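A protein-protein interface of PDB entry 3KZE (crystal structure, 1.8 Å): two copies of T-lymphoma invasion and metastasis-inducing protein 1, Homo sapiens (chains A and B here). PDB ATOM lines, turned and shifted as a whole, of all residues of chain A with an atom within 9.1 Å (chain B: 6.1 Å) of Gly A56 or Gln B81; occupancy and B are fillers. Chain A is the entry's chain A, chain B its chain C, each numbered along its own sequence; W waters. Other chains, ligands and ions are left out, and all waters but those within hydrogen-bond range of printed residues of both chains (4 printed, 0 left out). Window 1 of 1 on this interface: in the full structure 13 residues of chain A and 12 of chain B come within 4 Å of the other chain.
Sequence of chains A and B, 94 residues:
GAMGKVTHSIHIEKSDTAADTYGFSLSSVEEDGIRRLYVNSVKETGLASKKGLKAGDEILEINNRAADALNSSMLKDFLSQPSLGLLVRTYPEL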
ATOM      1  N   LYS A   5      21.022 -18.703  10.760  1.00  0.00           N
ATOM      2  CA  LYS A   5      19.861 -18.633   9.871  1.00  0.00           C
ATOM      3  C   LYS A   5      19.498 -20.013   9.342  1.00  0.00           C
ATOM      4  O   LYS A   5      20.336 -20.921   9.312  1.00  0.00           O
ATOM      5  CB  LYS A   5      20.150 -17.714   8.686  1.00  0.00           C
ATOM      6  CG  LYS A   5      20.467 -16.280   9.064  1.00  0.00           C
ATOM      7  CD  LYS A   5      20.781 -15.458   7.826  1.00  0.00           C
ATOM      8  CE  LYS A   5      21.068 -14.009   8.180  1.00  0.00           C
ATOM      9  NZ  LYS A   5      21.262 -13.172   6.953  1.00  0.00           N
ATOM     10  N   SER A  25       4.143  -7.360   3.669  1.00  0.00           N
ATOM     11  CA  SER A  25       4.711  -6.385   2.747  1.00  0.00           C
ATOM     12  C   SER A  25       6.219  -6.559   2.659  1.00  0.00           C
ATOM     13  O   SER A  25       6.842  -7.120   3.559  1.00  0.00           O
ATOM     14  CB  SER A  25       4.336  -4.950   3.143  1.00  0.00           C
ATOM     15  OG  SER A  25       4.985  -4.513   4.327  1.00  0.00           O
ATOM     16  N   LEU A  26       6.802  -6.070   1.573  1.00  0.00           N
ATOM     17  CA  LEU A  26       8.221  -6.275   1.320  1.00  0.00           C
ATOM     18  C   LEU A  26       8.950  -4.948   1.230  1.00  0.00           C
ATOM     19  O   LEU A  26       8.392  -3.957   0.744  1.00  0.00           O
ATOM     20  CB  LEU A  26       8.402  -7.054   0.016  1.00  0.00           C
ATOM     21  CG  LEU A  26       7.808  -8.463  -0.007  1.00  0.00           C
ATOM     22  CD1 LEU A  26       8.000  -9.103  -1.373  1.00  0.00           C
ATOM     23  CD2 LEU A  26       8.407  -9.336   1.090  1.00  0.00           C
ATOM     24  N   SER A  27      10.194  -4.941   1.699  1.00  0.00           N
ATOM     25  CA  SER A  27      11.084  -3.809   1.554  1.00  0.00           C
ATOM     26  C   SER A  27      12.284  -4.270   0.729  1.00  0.00           C
ATOM     27  O   SER A  27      12.583  -5.462   0.646  1.00  0.00           O
ATOM     28  CB  SER A  27      11.522  -3.297   2.927  1.00  0.00           C
ATOM     29  OG  SER A  27      12.202  -4.320   3.645  1.00  0.00           O
ATOM     30  N   SER A  28      12.968  -3.331   0.102  1.00  0.00           N
ATOM     31  CA  SER A  28      13.961  -3.698  -0.887  1.00  0.00           C
ATOM     32  C   SER A  28      15.257  -2.923  -0.657  1.00  0.00           C
ATOM     33  O   SER A  28      15.244  -1.774  -0.202  1.00  0.00           O
ATOM     34  CB  SER A  28      13.404  -3.411  -2.285  1.00  0.00           C
ATOM     35  OG  SER A  28      14.225  -3.929  -3.311  1.00  0.00           O
ATOM     36  N   VAL A  29      16.376  -3.561  -0.973  1.00  0.00           N
ATOM     37  CA  VAL A  29      17.662  -2.895  -0.942  1.00  0.00           C
ATOM     38  C   VAL A  29      18.572  -3.491  -2.007  1.00  0.00           C
ATOM     39  O   VAL A  29      18.626  -4.711  -2.192  1.00  0.00           O
ATOM     40  CB  VAL A  29      18.325  -2.979   0.453  1.00  0.00           C
ATOM     41  CG1 VAL A  29      18.509  -4.424   0.868  1.00  0.00           C
ATOM     42  CG2 VAL A  29      19.656  -2.237   0.452  1.00  0.00           C
ATOM     43  N   ARG A  36      17.945  -7.333  -2.883  1.00  0.00           N
ATOM     44  CA  ARG A  36      17.478  -8.263  -1.863  1.00  0.00           C
ATOM     45  C   ARG A  36      16.106  -7.820  -1.361  1.00  0.00           C
ATOM     46  O   ARG A  36      15.819  -6.618  -1.271  1.00  0.00           O
ATOM     47  CB  ARG A  36      18.479  -8.366  -0.698  1.00  0.00           C
ATOM     48  CG  ARG A  36      19.917  -8.617  -1.134  1.00  0.00           C
ATOM     49  CD  ARG A  36      20.890  -8.602   0.037  1.00  0.00           C
ATOM     50  NE  ARG A  36      20.803  -9.782   0.885  1.00  0.00           N
ATOM     51  CZ  ARG A  36      21.594  -9.982   1.938  1.00  0.00           C
ATOM     52  NH1 ARG A  36      22.505  -9.072   2.253  1.00  0.00           N
ATOM     53  NH2 ARG A  36      21.473 -11.076   2.682  1.00  0.00           N
ATOM     54  N   LEU A  37      15.253  -8.791  -1.044  1.00  0.00           N
ATOM     55  CA  LEU A  37      13.909  -8.491  -0.559  1.00  0.00           C
ATOM     56  C   LEU A  37      13.761  -8.966   0.861  1.00  0.00           C
ATOM     57  O   LEU A  37      14.174 -10.073   1.190  1.00  0.00           O
ATOM     58  CB  LEU A  37      12.847  -9.165  -1.433  1.00  0.00           C
ATOM     59  CG  LEU A  37      12.581  -8.570  -2.805  1.00  0.00           C
ATOM     60  CD1 LEU A  37      11.603  -9.464  -3.570  1.00  0.00           C
ATOM     61  CD2 LEU A  37      12.034  -7.147  -2.686  1.00  0.00           C
ATOM     62  N   TYR A  38      13.165  -8.123   1.698  1.00  0.00           N
ATOM     63  CA  TYR A  38      12.950  -8.446   3.093  1.00  0.00           C
ATOM     64  C   TYR A  38      11.499  -8.242   3.438  1.00  0.00           C
ATOM     65  O   TYR A  38      10.824  -7.382   2.872  1.00  0.00           O
ATOM     66  CB  TYR A  38      13.797  -7.551   4.000  1.00  0.00           C
ATOM     67  CG  TYR A  38      15.280  -7.838   3.926  1.00  0.00           C
ATOM     68  CD1 TYR A  38      15.854  -8.845   4.703  1.00  0.00           C
ATOM     69  CD2 TYR A  38      16.095  -7.122   3.070  1.00  0.00           C
ATOM     70  CE1 TYR A  38      17.200  -9.113   4.631  1.00  0.00           C
ATOM     71  CE2 TYR A  38      17.457  -7.374   2.999  1.00  0.00           C
ATOM     72  CZ  TYR A  38      17.997  -8.376   3.777  1.00  0.00           C
ATOM     73  OH  TYR A  38      19.332  -8.644   3.702  1.00  0.00           O
ATOM     74  N   VAL A  39      11.022  -9.047   4.373  1.00  0.00           N
ATOM     75  CA  VAL A  39       9.693  -8.864   4.907  1.00  0.00           C
ATOM     76  C   VAL A  39       9.664  -7.649   5.818  1.00  0.00           C
ATOM     77  O   VAL A  39      10.364  -7.575   6.847  1.00  0.00           O
ATOM     78  CB  VAL A  39       9.219 -10.112   5.656  1.00  0.00           C
ATOM     79  CG1 VAL A  39       7.844  -9.861   6.211  1.00  0.00           C
ATOM     80  CG2 VAL A  39       9.223 -11.330   4.695  1.00  0.00           C
ATOM     81  N   ASN A  40       8.864  -6.676   5.401  1.00  0.00           N
ATOM     82  CA  ASN A  40       8.742  -5.404   6.076  1.00  0.00           C
ATOM     83  C   ASN A  40       7.796  -5.522   7.259  1.00  0.00           C
ATOM     84  O   ASN A  40       8.107  -5.085   8.371  1.00  0.00           O
ATOM     85  CB  ASN A  40       8.225  -4.375   5.070  1.00  0.00           C
ATOM     86  CG  ASN A  40       8.020  -3.018   5.678  1.00  0.00           C
ATOM     87  OD1 ASN A  40       8.494  -2.737   6.767  1.00  0.00           O
ATOM     88  ND2 ASN A  40       7.301  -2.163   4.971  1.00  0.00           N
ATOM     89  N   SER A  41       6.639  -6.124   7.018  1.00  0.00           N
ATOM     90  CA  SER A  41       5.650  -6.312   8.062  1.00  0.00           C
ATOM     91  C   SER A  41       4.805  -7.552   7.789  1.00  0.00           C
ATOM     92  O   SER A  41       4.588  -7.925   6.637  1.00  0.00           O
ATOM     93  CB  SER A  41       4.749  -5.081   8.156  1.00  0.00           C
ATOM     94  OG  SER A  41       3.976  -4.933   6.977  1.00  0.00           O
ATOM     95  N   VAL A  42       4.347  -8.195   8.857  1.00  0.00           N
ATOM     96  CA  VAL A  42       3.429  -9.326   8.742  1.00  0.00           C
ATOM     97  C   VAL A  42       2.193  -9.034   9.574  1.00  0.00           C
ATOM     98  O   VAL A  42       2.299  -8.643  10.748  1.00  0.00           O
ATOM     99  CB  VAL A  42       4.091 -10.650   9.191  1.00  0.00           C
ATOM    100  CG1 VAL A  42       3.107 -11.793   9.113  1.00  0.00           C
ATOM    101  CG2 VAL A  42       5.341 -10.946   8.324  1.00  0.00           C
ATOM    102  N   LEU A  53       5.633 -16.853   8.170  1.00  0.00           N
ATOM    103  CA  LEU A  53       6.462 -15.763   7.660  1.00  0.00           C
ATOM    104  C   LEU A  53       6.666 -14.732   8.779  1.00  0.00           C
ATOM    105  O   LEU A  53       5.731 -14.413   9.523  1.00  0.00           O
ATOM    106  CB  LEU A  53       5.843 -15.137   6.399  1.00  0.00           C
ATOM    107  CG  LEU A  53       6.741 -14.165   5.633  1.00  0.00           C
ATOM    108  CD1 LEU A  53       7.900 -14.922   4.959  1.00  0.00           C
ATOM    109  CD2 LEU A  53       5.943 -13.349   4.612  1.00  0.00           C
ATOM    110  N   LYS A  54       7.900 -14.248   8.918  1.00  0.00           N
ATOM    111  CA  LYS A  54       8.264 -13.313   9.992  1.00  0.00           C
ATOM    112  C   LYS A  54       8.835 -11.998   9.473  1.00  0.00           C
ATOM    113  O   LYS A  54       9.565 -11.971   8.472  1.00  0.00           O
ATOM    114  CB  LYS A  54       9.305 -13.943  10.927  1.00  0.00           C
ATOM    115  CG  LYS A  54       9.005 -15.366  11.393  1.00  0.00           C
ATOM    116  CD  LYS A  54       7.837 -15.393  12.344  1.00  0.00           C
ATOM    117  CE  LYS A  54       7.516 -16.814  12.787  1.00  0.00           C
ATOM    118  NZ  LYS A  54       8.630 -17.407  13.563  1.00  0.00           N
ATOM    119  N   ALA A  55       8.517 -10.906  10.166  1.00  0.00           N
ATOM    120  CA  ALA A  55       9.159  -9.626   9.895  1.00  0.00           C
ATOM    121  C   ALA A  55      10.683  -9.767  10.002  1.00  0.00           C
ATOM    122  O   ALA A  55      11.212 -10.361  10.954  1.00  0.00           O
ATOM    123  CB  ALA A  55       8.655  -8.565  10.863  1.00  0.00           C
ATOM    124  N   GLY A  56      11.390  -9.218   9.024  1.00  0.00           N
ATOM    125  CA  GLY A  56      12.837  -9.305   9.025  1.00  0.00           C
ATOM    126  C   GLY A  56      13.367 -10.519   8.291  1.00  0.00           C
ATOM    127  O   GLY A  56      14.572 -10.636   8.086  1.00  0.00           O
ATOM    128  N   ASP A  57      12.477 -11.442   7.910  1.00  0.00           N
ATOM    129  CA  ASP A  57      12.869 -12.552   7.035  1.00  0.00           C
ATOM    130  C   ASP A  57      13.373 -12.031   5.699  1.00  0.00           C
ATOM    131  O   ASP A  57      12.925 -10.982   5.220  1.00  0.00           O
ATOM    132  CB  ASP A  57      11.697 -13.495   6.765  1.00  0.00           C
ATOM    133  CG  ASP A  57      11.404 -14.423   7.918  1.00  0.00           C
ATOM    134  OD1 ASP A  57      12.114 -14.369   8.946  1.00  0.00           O
ATOM    135  OD2 ASP A  57      10.453 -15.233   7.777  1.00  0.00           O
ATOM    136  N   GLU A  58      14.303 -12.752   5.090  1.00  0.00           N
ATOM    137  CA  GLU A  58      14.713 -12.423   3.723  1.00  0.00           C
ATOM    138  C   GLU A  58      13.989 -13.321   2.740  1.00  0.00           C
ATOM    139  O   GLU A  58      13.882 -14.530   2.962  1.00  0.00           O
ATOM    140  CB  GLU A  58      16.228 -12.551   3.522  1.00  0.00           C
ATOM    141  CG  GLU A  58      16.679 -12.078   2.142  1.00  0.00           C
ATOM    142  CD  GLU A  58      18.174 -12.158   1.907  1.00  0.00           C
ATOM    143  OE1 GLU A  58      18.924 -12.569   2.827  1.00  0.00           O
ATOM    144  OE2 GLU A  58      18.598 -11.811   0.779  1.00  0.00           O
ATOM    145  N   ILE A  59      13.472 -12.738   1.656  1.00  0.00           N
ATOM    146  CA  ILE A  59      12.858 -13.534   0.595  1.00  0.00           C
ATOM    147  C   ILE A  59      13.908 -13.836  -0.464  1.00  0.00           C
ATOM    148  O   ILE A  59      14.387 -12.926  -1.148  1.00  0.00           O
ATOM    149  CB  ILE A  59      11.659 -12.811  -0.092  1.00  0.00           C
ATOM    150  CG1 ILE A  59      10.608 -12.396   0.939  1.00  0.00           C
ATOM    151  CG2 ILE A  59      11.041 -13.707  -1.204  1.00  0.00           C
ATOM    152  CD1 ILE A  59       9.980 -13.540   1.691  1.00  0.00           C
ATOM    153  N   VAL A  88      12.429 -18.699   1.847  1.00  0.00           N
ATOM    154  CA  VAL A  88      12.602 -17.724   2.915  1.00  0.00           C
ATOM    155  C   VAL A  88      13.797 -18.073   3.784  1.00  0.00           C
ATOM    156  O   VAL A  88      14.014 -19.237   4.128  1.00  0.00           O
ATOM    157  CB  VAL A  88      11.344 -17.705   3.824  1.00  0.00           C
ATOM    158  CG1 VAL A  88      11.450 -16.619   4.876  1.00  0.00           C
ATOM    159  CG2 VAL A  88      10.088 -17.519   2.995  1.00  0.00           C
ATOM    160  N   ARG A  89      14.555 -17.056   4.167  1.00  0.00           N
ATOM    161  CA  ARG A  89      15.640 -17.217   5.126  1.00  0.00           C
ATOM    162  C   ARG A  89      15.267 -16.485   6.417  1.00  0.00           C
ATOM    163  O   ARG A  89      14.940 -15.294   6.409  1.00  0.00           O
ATOM    164  CB  ARG A  89      16.941 -16.676   4.541  1.00  0.00           C
ATOM    165  CG  ARG A  89      18.169 -16.973   5.374  1.00  0.00           C
ATOM    166  CD  ARG A  89      19.403 -17.090   4.487  1.00  0.00           C
ATOM    167  NE  ARG A  89      19.807 -15.812   3.900  1.00  0.00           N
ATOM    168  CZ  ARG A  89      20.634 -15.693   2.861  1.00  0.00           C
ATOM    169  NH1 ARG A  89      20.959 -14.488   2.412  1.00  0.00           N
ATOM    170  NH2 ARG A  89      21.147 -16.784   2.277  1.00  0.00           N
ATOM    171  N   THR A  90      15.333 -17.198   7.537  1.00  0.00           N
ATOM    172  CA  THR A  90      14.808 -16.698   8.792  1.00  0.00           C
ATOM    173  C   THR A  90      15.724 -17.110   9.947  1.00  0.00           C
ATOM    174  O   THR A  90      16.603 -17.958   9.785  1.00  0.00           O
ATOM    175  CB  THR A  90      13.373 -17.254   9.039  1.00  0.00           C
ATOM    176  OG1 THR A  90      12.755 -16.592  10.151  1.00  0.00           O
ATOM    177  CG2 THR A  90      13.409 -18.768   9.289  1.00  0.00           C
ATOM    178  N   TYR A  91      15.531 -16.494  11.096  1.00  0.00           N
ATOM    179  CA  TYR A  91      16.156 -17.005  12.318  1.00  0.00           C
ATOM    180  C   TYR A  91      15.136 -17.839  13.068  1.00  0.00           C
ATOM    181  O   TYR A  91      13.981 -17.431  13.222  1.00  0.00           O
ATOM    182  CB  TYR A  91      16.627 -15.886  13.220  1.00  0.00           C
ATOM    183  CG  TYR A  91      17.708 -15.016  12.626  1.00  0.00           C
ATOM    184  CD1 TYR A  91      19.046 -15.369  12.729  1.00  0.00           C
ATOM    185  CD2 TYR A  91      17.387 -13.829  11.977  1.00  0.00           C
ATOM    186  CE1 TYR A  91      20.040 -14.559  12.189  1.00  0.00           C
ATOM    187  CE2 TYR A  91      18.358 -13.029  11.442  1.00  0.00           C
ATOM    188  CZ  TYR A  91      19.686 -13.400  11.540  1.00  0.00           C
ATOM    189  OH  TYR A  91      20.655 -12.586  10.994  1.00  0.00           O
ATOM    190  N   LYS B  14      14.373   2.838   5.403  1.00  0.00           N
ATOM    191  CA  LYS B  14      15.501   3.531   4.807  1.00  0.00           C
ATOM    192  C   LYS B  14      15.384   3.448   3.295  1.00  0.00           C
ATOM    193  O   LYS B  14      15.040   2.400   2.753  1.00  0.00           O
ATOM    194  CB  LYS B  14      16.818   2.891   5.240  1.00  0.00           C
ATOM    195  CG  LYS B  14      17.111   2.994   6.714  1.00  0.00           C
ATOM    196  CD  LYS B  14      18.497   2.457   7.016  1.00  0.00           C
ATOM    197  CE  LYS B  14      18.676   1.064   6.459  1.00  0.00           C
ATOM    198  NZ  LYS B  14      20.064   0.589   6.651  1.00  0.00           N
ATOM    199  N   TYR B  22      20.161   4.036  10.687  1.00  0.00           N
ATOM    200  CA  TYR B  22      18.928   4.476  11.349  1.00  0.00           C
ATOM    201  C   TYR B  22      19.186   5.584  12.370  1.00  0.00           C
ATOM    202  O   TYR B  22      18.251   6.180  12.907  1.00  0.00           O
ATOM    203  CB  TYR B  22      18.163   3.297  11.990  1.00  0.00           C
ATOM    204  CG  TYR B  22      17.427   2.422  11.000  1.00  0.00           C
ATOM    205  CD1 TYR B  22      16.283   2.884  10.344  1.00  0.00           C
ATOM    206  CD2 TYR B  22      17.858   1.124  10.728  1.00  0.00           C
ATOM    207  CE1 TYR B  22      15.606   2.087   9.449  1.00  0.00           C
ATOM    208  CE2 TYR B  22      17.178   0.318   9.823  1.00  0.00           C
ATOM    209  CZ  TYR B  22      16.057   0.810   9.185  1.00  0.00           C
ATOM    210  OH  TYR B  22      15.374   0.034   8.279  1.00  0.00           O
ATOM    211  N   ASN B  63      11.225  -6.340  15.424  1.00  0.00           N
ATOM    212  CA  ASN B  63      10.546  -7.197  14.453  1.00  0.00           C
ATOM    213  C   ASN B  63       9.712  -8.287  15.125  1.00  0.00           C
ATOM    214  O   ASN B  63       9.698  -9.435  14.681  1.00  0.00           O
ATOM    215  CB  ASN B  63      11.554  -7.780  13.454  1.00  0.00           C
ATOM    216  CG  ASN B  63      12.172  -6.706  12.567  1.00  0.00           C
ATOM    217  OD1 ASN B  63      11.611  -5.617  12.426  1.00  0.00           O
ATOM    218  ND2 ASN B  63      13.323  -7.006  11.965  1.00  0.00           N
ATOM    219  N   LYS B  76      22.466  -7.282  14.440  1.00  0.00           N
ATOM    220  CA  LYS B  76      23.226  -6.693  13.353  1.00  0.00           C
ATOM    221  C   LYS B  76      22.461  -6.773  12.041  1.00  0.00           C
ATOM    222  O   LYS B  76      22.419  -5.808  11.292  1.00  0.00           O
ATOM    223  CB  LYS B  76      24.589  -7.377  13.227  1.00  0.00           C
ATOM    224  CG  LYS B  76      25.497  -7.130  14.416  1.00  0.00           C
ATOM    225  CD  LYS B  76      26.760  -7.974  14.340  1.00  0.00           C
ATOM    226  CE  LYS B  76      27.603  -7.815  15.595  1.00  0.00           C
ATOM    227  NZ  LYS B  76      28.027  -6.402  15.788  1.00  0.00           N
ATOM    228  N   ASP B  77      21.850  -7.924  11.771  1.00  0.00           N
ATOM    229  CA  ASP B  77      21.072  -8.095  10.552  1.00  0.00           C
ATOM    230  C   ASP B  77      19.874  -7.140  10.548  1.00  0.00           C
ATOM    231  O   ASP B  77      19.713  -6.326   9.627  1.00  0.00           O
ATOM    232  CB  ASP B  77      20.613  -9.557  10.419  1.00  0.00           C
ATOM    233  CG  ASP B  77      19.851  -9.822   9.133  1.00  0.00           C
ATOM    234  OD1 ASP B  77      19.669  -8.892   8.311  1.00  0.00           O
ATOM    235  OD2 ASP B  77      19.426 -10.972   8.936  1.00  0.00           O
ATOM    236  N   PHE B  78      19.037  -7.228  11.578  1.00  0.00           N
ATOM    237  CA  PHE B  78      17.850  -6.370  11.653  1.00  0.00           C
ATOM    238  C   PHE B  78      18.173  -4.872  11.568  1.00  0.00           C
ATOM    239  O   PHE B  78      17.469  -4.129  10.895  1.00  0.00           O
ATOM    240  CB  PHE B  78      17.021  -6.661  12.908  1.00  0.00           C
ATOM    241  CG  PHE B  78      16.365  -8.012  12.905  1.00  0.00           C
ATOM    242  CD1 PHE B  78      16.276  -8.747  11.734  1.00  0.00           C
ATOM    243  CD2 PHE B  78      15.818  -8.536  14.062  1.00  0.00           C
ATOM    244  CE1 PHE B  78      15.658  -9.983  11.707  1.00  0.00           C
ATOM    245  CE2 PHE B  78      15.193  -9.782  14.043  1.00  0.00           C
ATOM    246  CZ  PHE B  78      15.124 -10.506  12.866  1.00  0.00           C
ATOM    247  N   LEU B  79      19.224  -4.426  12.245  1.00  0.00           N
ATOM    248  CA  LEU B  79      19.537  -2.998  12.271  1.00  0.00           C
ATOM    249  C   LEU B  79      20.070  -2.493  10.935  1.00  0.00           C
ATOM    250  O   LEU B  79      20.141  -1.284  10.709  1.00  0.00           O
ATOM    251  CB  LEU B  79      20.522  -2.675  13.390  1.00  0.00           C
ATOM    252  CG  LEU B  79      19.961  -3.013  14.769  1.00  0.00           C
ATOM    253  CD1 LEU B  79      20.964  -2.700  15.884  1.00  0.00           C
ATOM    254  CD2 LEU B  79      18.661  -2.274  14.989  1.00  0.00           C
ATOM    255  N   SER B  80      20.423  -3.412  10.044  1.00  0.00           N
ATOM    256  CA  SER B  80      20.981  -3.020   8.752  1.00  0.00           C
ATOM    257  C   SER B  80      19.999  -3.188   7.591  1.00  0.00           C
ATOM    258  O   SER B  80      20.316  -2.835   6.454  1.00  0.00           O
ATOM    259  CB  SER B  80      22.283  -3.778   8.474  1.00  0.00           C
ATOM    260  OG  SER B  80      22.052  -5.159   8.284  1.00  0.00           O
ATOM    261  N   GLN B  81      18.812  -3.720   7.879  1.00  0.00           N
ATOM    262  CA  GLN B  81      17.784  -3.932   6.848  1.00  0.00           C
ATOM    263  C   GLN B  81      17.107  -2.627   6.466  1.00  0.00           C
ATOM    264  O   GLN B  81      17.121  -1.672   7.257  1.00  0.00           O
ATOM    265  CB  GLN B  81      16.722  -4.915   7.342  1.00  0.00           C
ATOM    266  CG  GLN B  81      17.211  -6.357   7.357  1.00  0.00           C
ATOM    267  CD  GLN B  81      16.112  -7.362   7.668  1.00  0.00           C
ATOM    268  OE1 GLN B  81      14.913  -7.088   7.501  1.00  0.00           O
ATOM    269  NE2 GLN B  81      16.519  -8.535   8.126  1.00  0.00           N
ATOM    270  N   PRO B  82      16.476  -2.596   5.278  1.00  0.00           N
ATOM    271  CA  PRO B  82      15.839  -1.384   4.743  1.00  0.00           C
ATOM    272  C   PRO B  82      14.540  -0.993   5.458  1.00  0.00           C
ATOM    273  O   PRO B  82      14.011   0.109   5.239  1.00  0.00           O
ATOM    274  CB  PRO B  82      15.574  -1.731   3.277  1.00  0.00           C
ATOM    275  CG  PRO B  82      15.585  -3.247   3.209  1.00  0.00           C
ATOM    276  CD  PRO B  82      16.461  -3.724   4.318  1.00  0.00           C
ATOM    277  N   SER B  83      14.026  -1.883   6.294  1.00  0.00           N
ATOM    278  CA  SER B  83      12.937  -1.520   7.202  1.00  0.00           C
ATOM    279  C   SER B  83      13.145  -2.161   8.574  1.00  0.00           C
ATOM    280  O   SER B  83      13.776  -3.217   8.692  1.00  0.00           O
ATOM    281  CB  SER B  83      11.583  -1.929   6.628  1.00  0.00           C
ATOM    282  OG  SER B  83      11.476  -3.341   6.568  1.00  0.00           O
ATOM    283  N   LEU B  84      12.589  -1.530   9.603  1.00  0.00           N
ATOM    284  CA  LEU B  84      12.805  -1.966  10.980  1.00  0.00           C
ATOM    285  C   LEU B  84      11.580  -1.685  11.822  1.00  0.00           C
ATOM    286  O   LEU B  84      11.036  -0.590  11.787  1.00  0.00           O
ATOM    287  CB  LEU B  84      13.990  -1.211  11.572  1.00  0.00           C
ATOM    288  CG  LEU B  84      14.336  -1.459  13.033  1.00  0.00           C
ATOM    289  CD1 LEU B  84      14.858  -2.878  13.217  1.00  0.00           C
ATOM    290  CD2 LEU B  84      15.371  -0.438  13.473  1.00  0.00           C
HETATM  291  O   HOH W   1      10.700 -11.551  13.382  1.00  0.00           O
HETATM  292  O   HOH W   2      20.188 -10.420   5.796  1.00  0.00           O
HETATM  293  O   HOH W   3      16.725 -11.852   9.025  1.00  0.00           O
HETATM  294  O   HOH W   4      10.134  -4.842  10.214  1.00  0.00           O
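The side-chain hydroxyl (OH) of Tyr A91 lies within hydrogen-bond range of the side-chain carboxylate (OD2) of Asp B77 (2.9 Å). The side-chain amide nitrogen of Gln B81 sits at hydrogen-bond distance from the backbone carbonyl oxygen of Gly A56 (2.9 Å). OG of Ser B83 lies within hydrogen-bond range of OD1 of Asn A40 (3.0 Å). The side-chain hydroxyl (OG) of Ser A27 lies within hydrogen-bond range of the side-chain hydroxyl (OG) of Ser B83 (3.2 Å). The side-chain carboxylate (OD2) of Asp B77 lies within salt-bridge range of the side-chain amino group (NZ) of Lys A5 (3.5 Å).
The backbone carbonyl oxygen (O) of Asp B77 sits at hydrogen-bond distance from the side-chain hydroxyl (OG) of Ser B80 (2.9 Å). The side-chain carboxylate (OD1) of Asp B77 is in hydrogen-bond range of the side-chain amide nitrogen (NE2) of Gln B81 (3.2 Å). N of Arg A36 sits at hydrogen-bond distance from O of Val A29. The side-chain hydroxyl (OH) of Tyr B22 sits at hydrogen-bond distance from the backbone carbonyl oxygen (O) of Gln B81. The backbone carbonyl oxygen (O) of Ser A25 is in hydrogen-bond range of the backbone NH (N) of Asn A40, 2.8 Å away. The guanidinium group (NE) of Arg A36 lies close to the side-chain hydroxyl (OH) of Tyr A38, at 3.4 Å.
Ser A27 touches Pro B82. Ser A28 touches Pro B82. Val A29 touches Pro B82. Tyr A38 touches Gln B81 (CD1 to CD, 3.3 Å). CD2 of Tyr A38 touches CD of Pro B82 (3.6 Å). Ala A55 touches Asn B63. Gly A56 touches Asn B63. Gly A56 touches Phe B78.
Of the printed residues of chain B, Ser A27 touches Pro B82 and Ser B83. Printed residues of chain B within 4 Å of Tyr A38: Gln B81 (3.3 Å) and Pro B82 (3.6 Å). Of the printed residues of chain B, Gly A56 touches Asn B63, Phe B78 and Gln B81. Of the printed residues of chain A, Phe B78 touches Gly A56 (3.8 Å). Ser B80 touches none of the printed residues of chain A. Gln B81 touches just these residues of chain A: Tyr A38 (3.3 Å) and Gly A56 (2.9 Å). Pro B82 touches four residues of chain A. Of the printed residues of chain A, Ser B83 touches Ser A27 and Asn A40. The nearest residue of chain A that does not touch Gln B81 is Val A39 (4.6 Å).
Of the 24 printed residues of chain A, 9 touch a printed residue of chain B. Printed residues of chain A that touch a printed residue of chain B: Lys A5, Ser A27, Ser A28, Val A29, Tyr A38, Asn A40, Ala A55, Gly A56 and Tyr A91. Hydrophobic or aromatic side chains of chain A within 4 Å of the printed part of chain B: Val A29, Tyr A38, Ala A55 and Tyr A91. Printed residues of chain B that touch a printed residue of chain A: Asn B63, Asp B77, Phe B78, Gln B81, Pro B82 and Ser B83. Along chain B the printed residues that touch a printed residue of chain A span positions 63 to 83. Among the printed residues, 13 pairs touch across the chains.
No position is printed for both chains. Of the 13 pairs that touch across the chains among the printed residues, none has its exchanged pair printed and touching as well.
Water W3 lies within hydrogen-bond range of O of Gly A56 (2.6 Å), OD2 of Asp B77 (2.8 Å) and NE2 of Gln B81 (3.4 Å). Water W1 bridges the backbone carbonyl oxygen (O) of Asn B63 (2.7 Å) and the backbone carbonyl oxygen (O) of Ala A55 (2.8 Å). Water W4 bridges O of Asn A40 and OD1 of Asn B63. Water W2 lies within hydrogen-bond range of OH of Tyr A38 (2.9 Å), OD1 of Asp B77 (3.0 Å), NZ of Lys A5 (3.2 Å) and NH2 of Arg A36 (3.4 Å).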
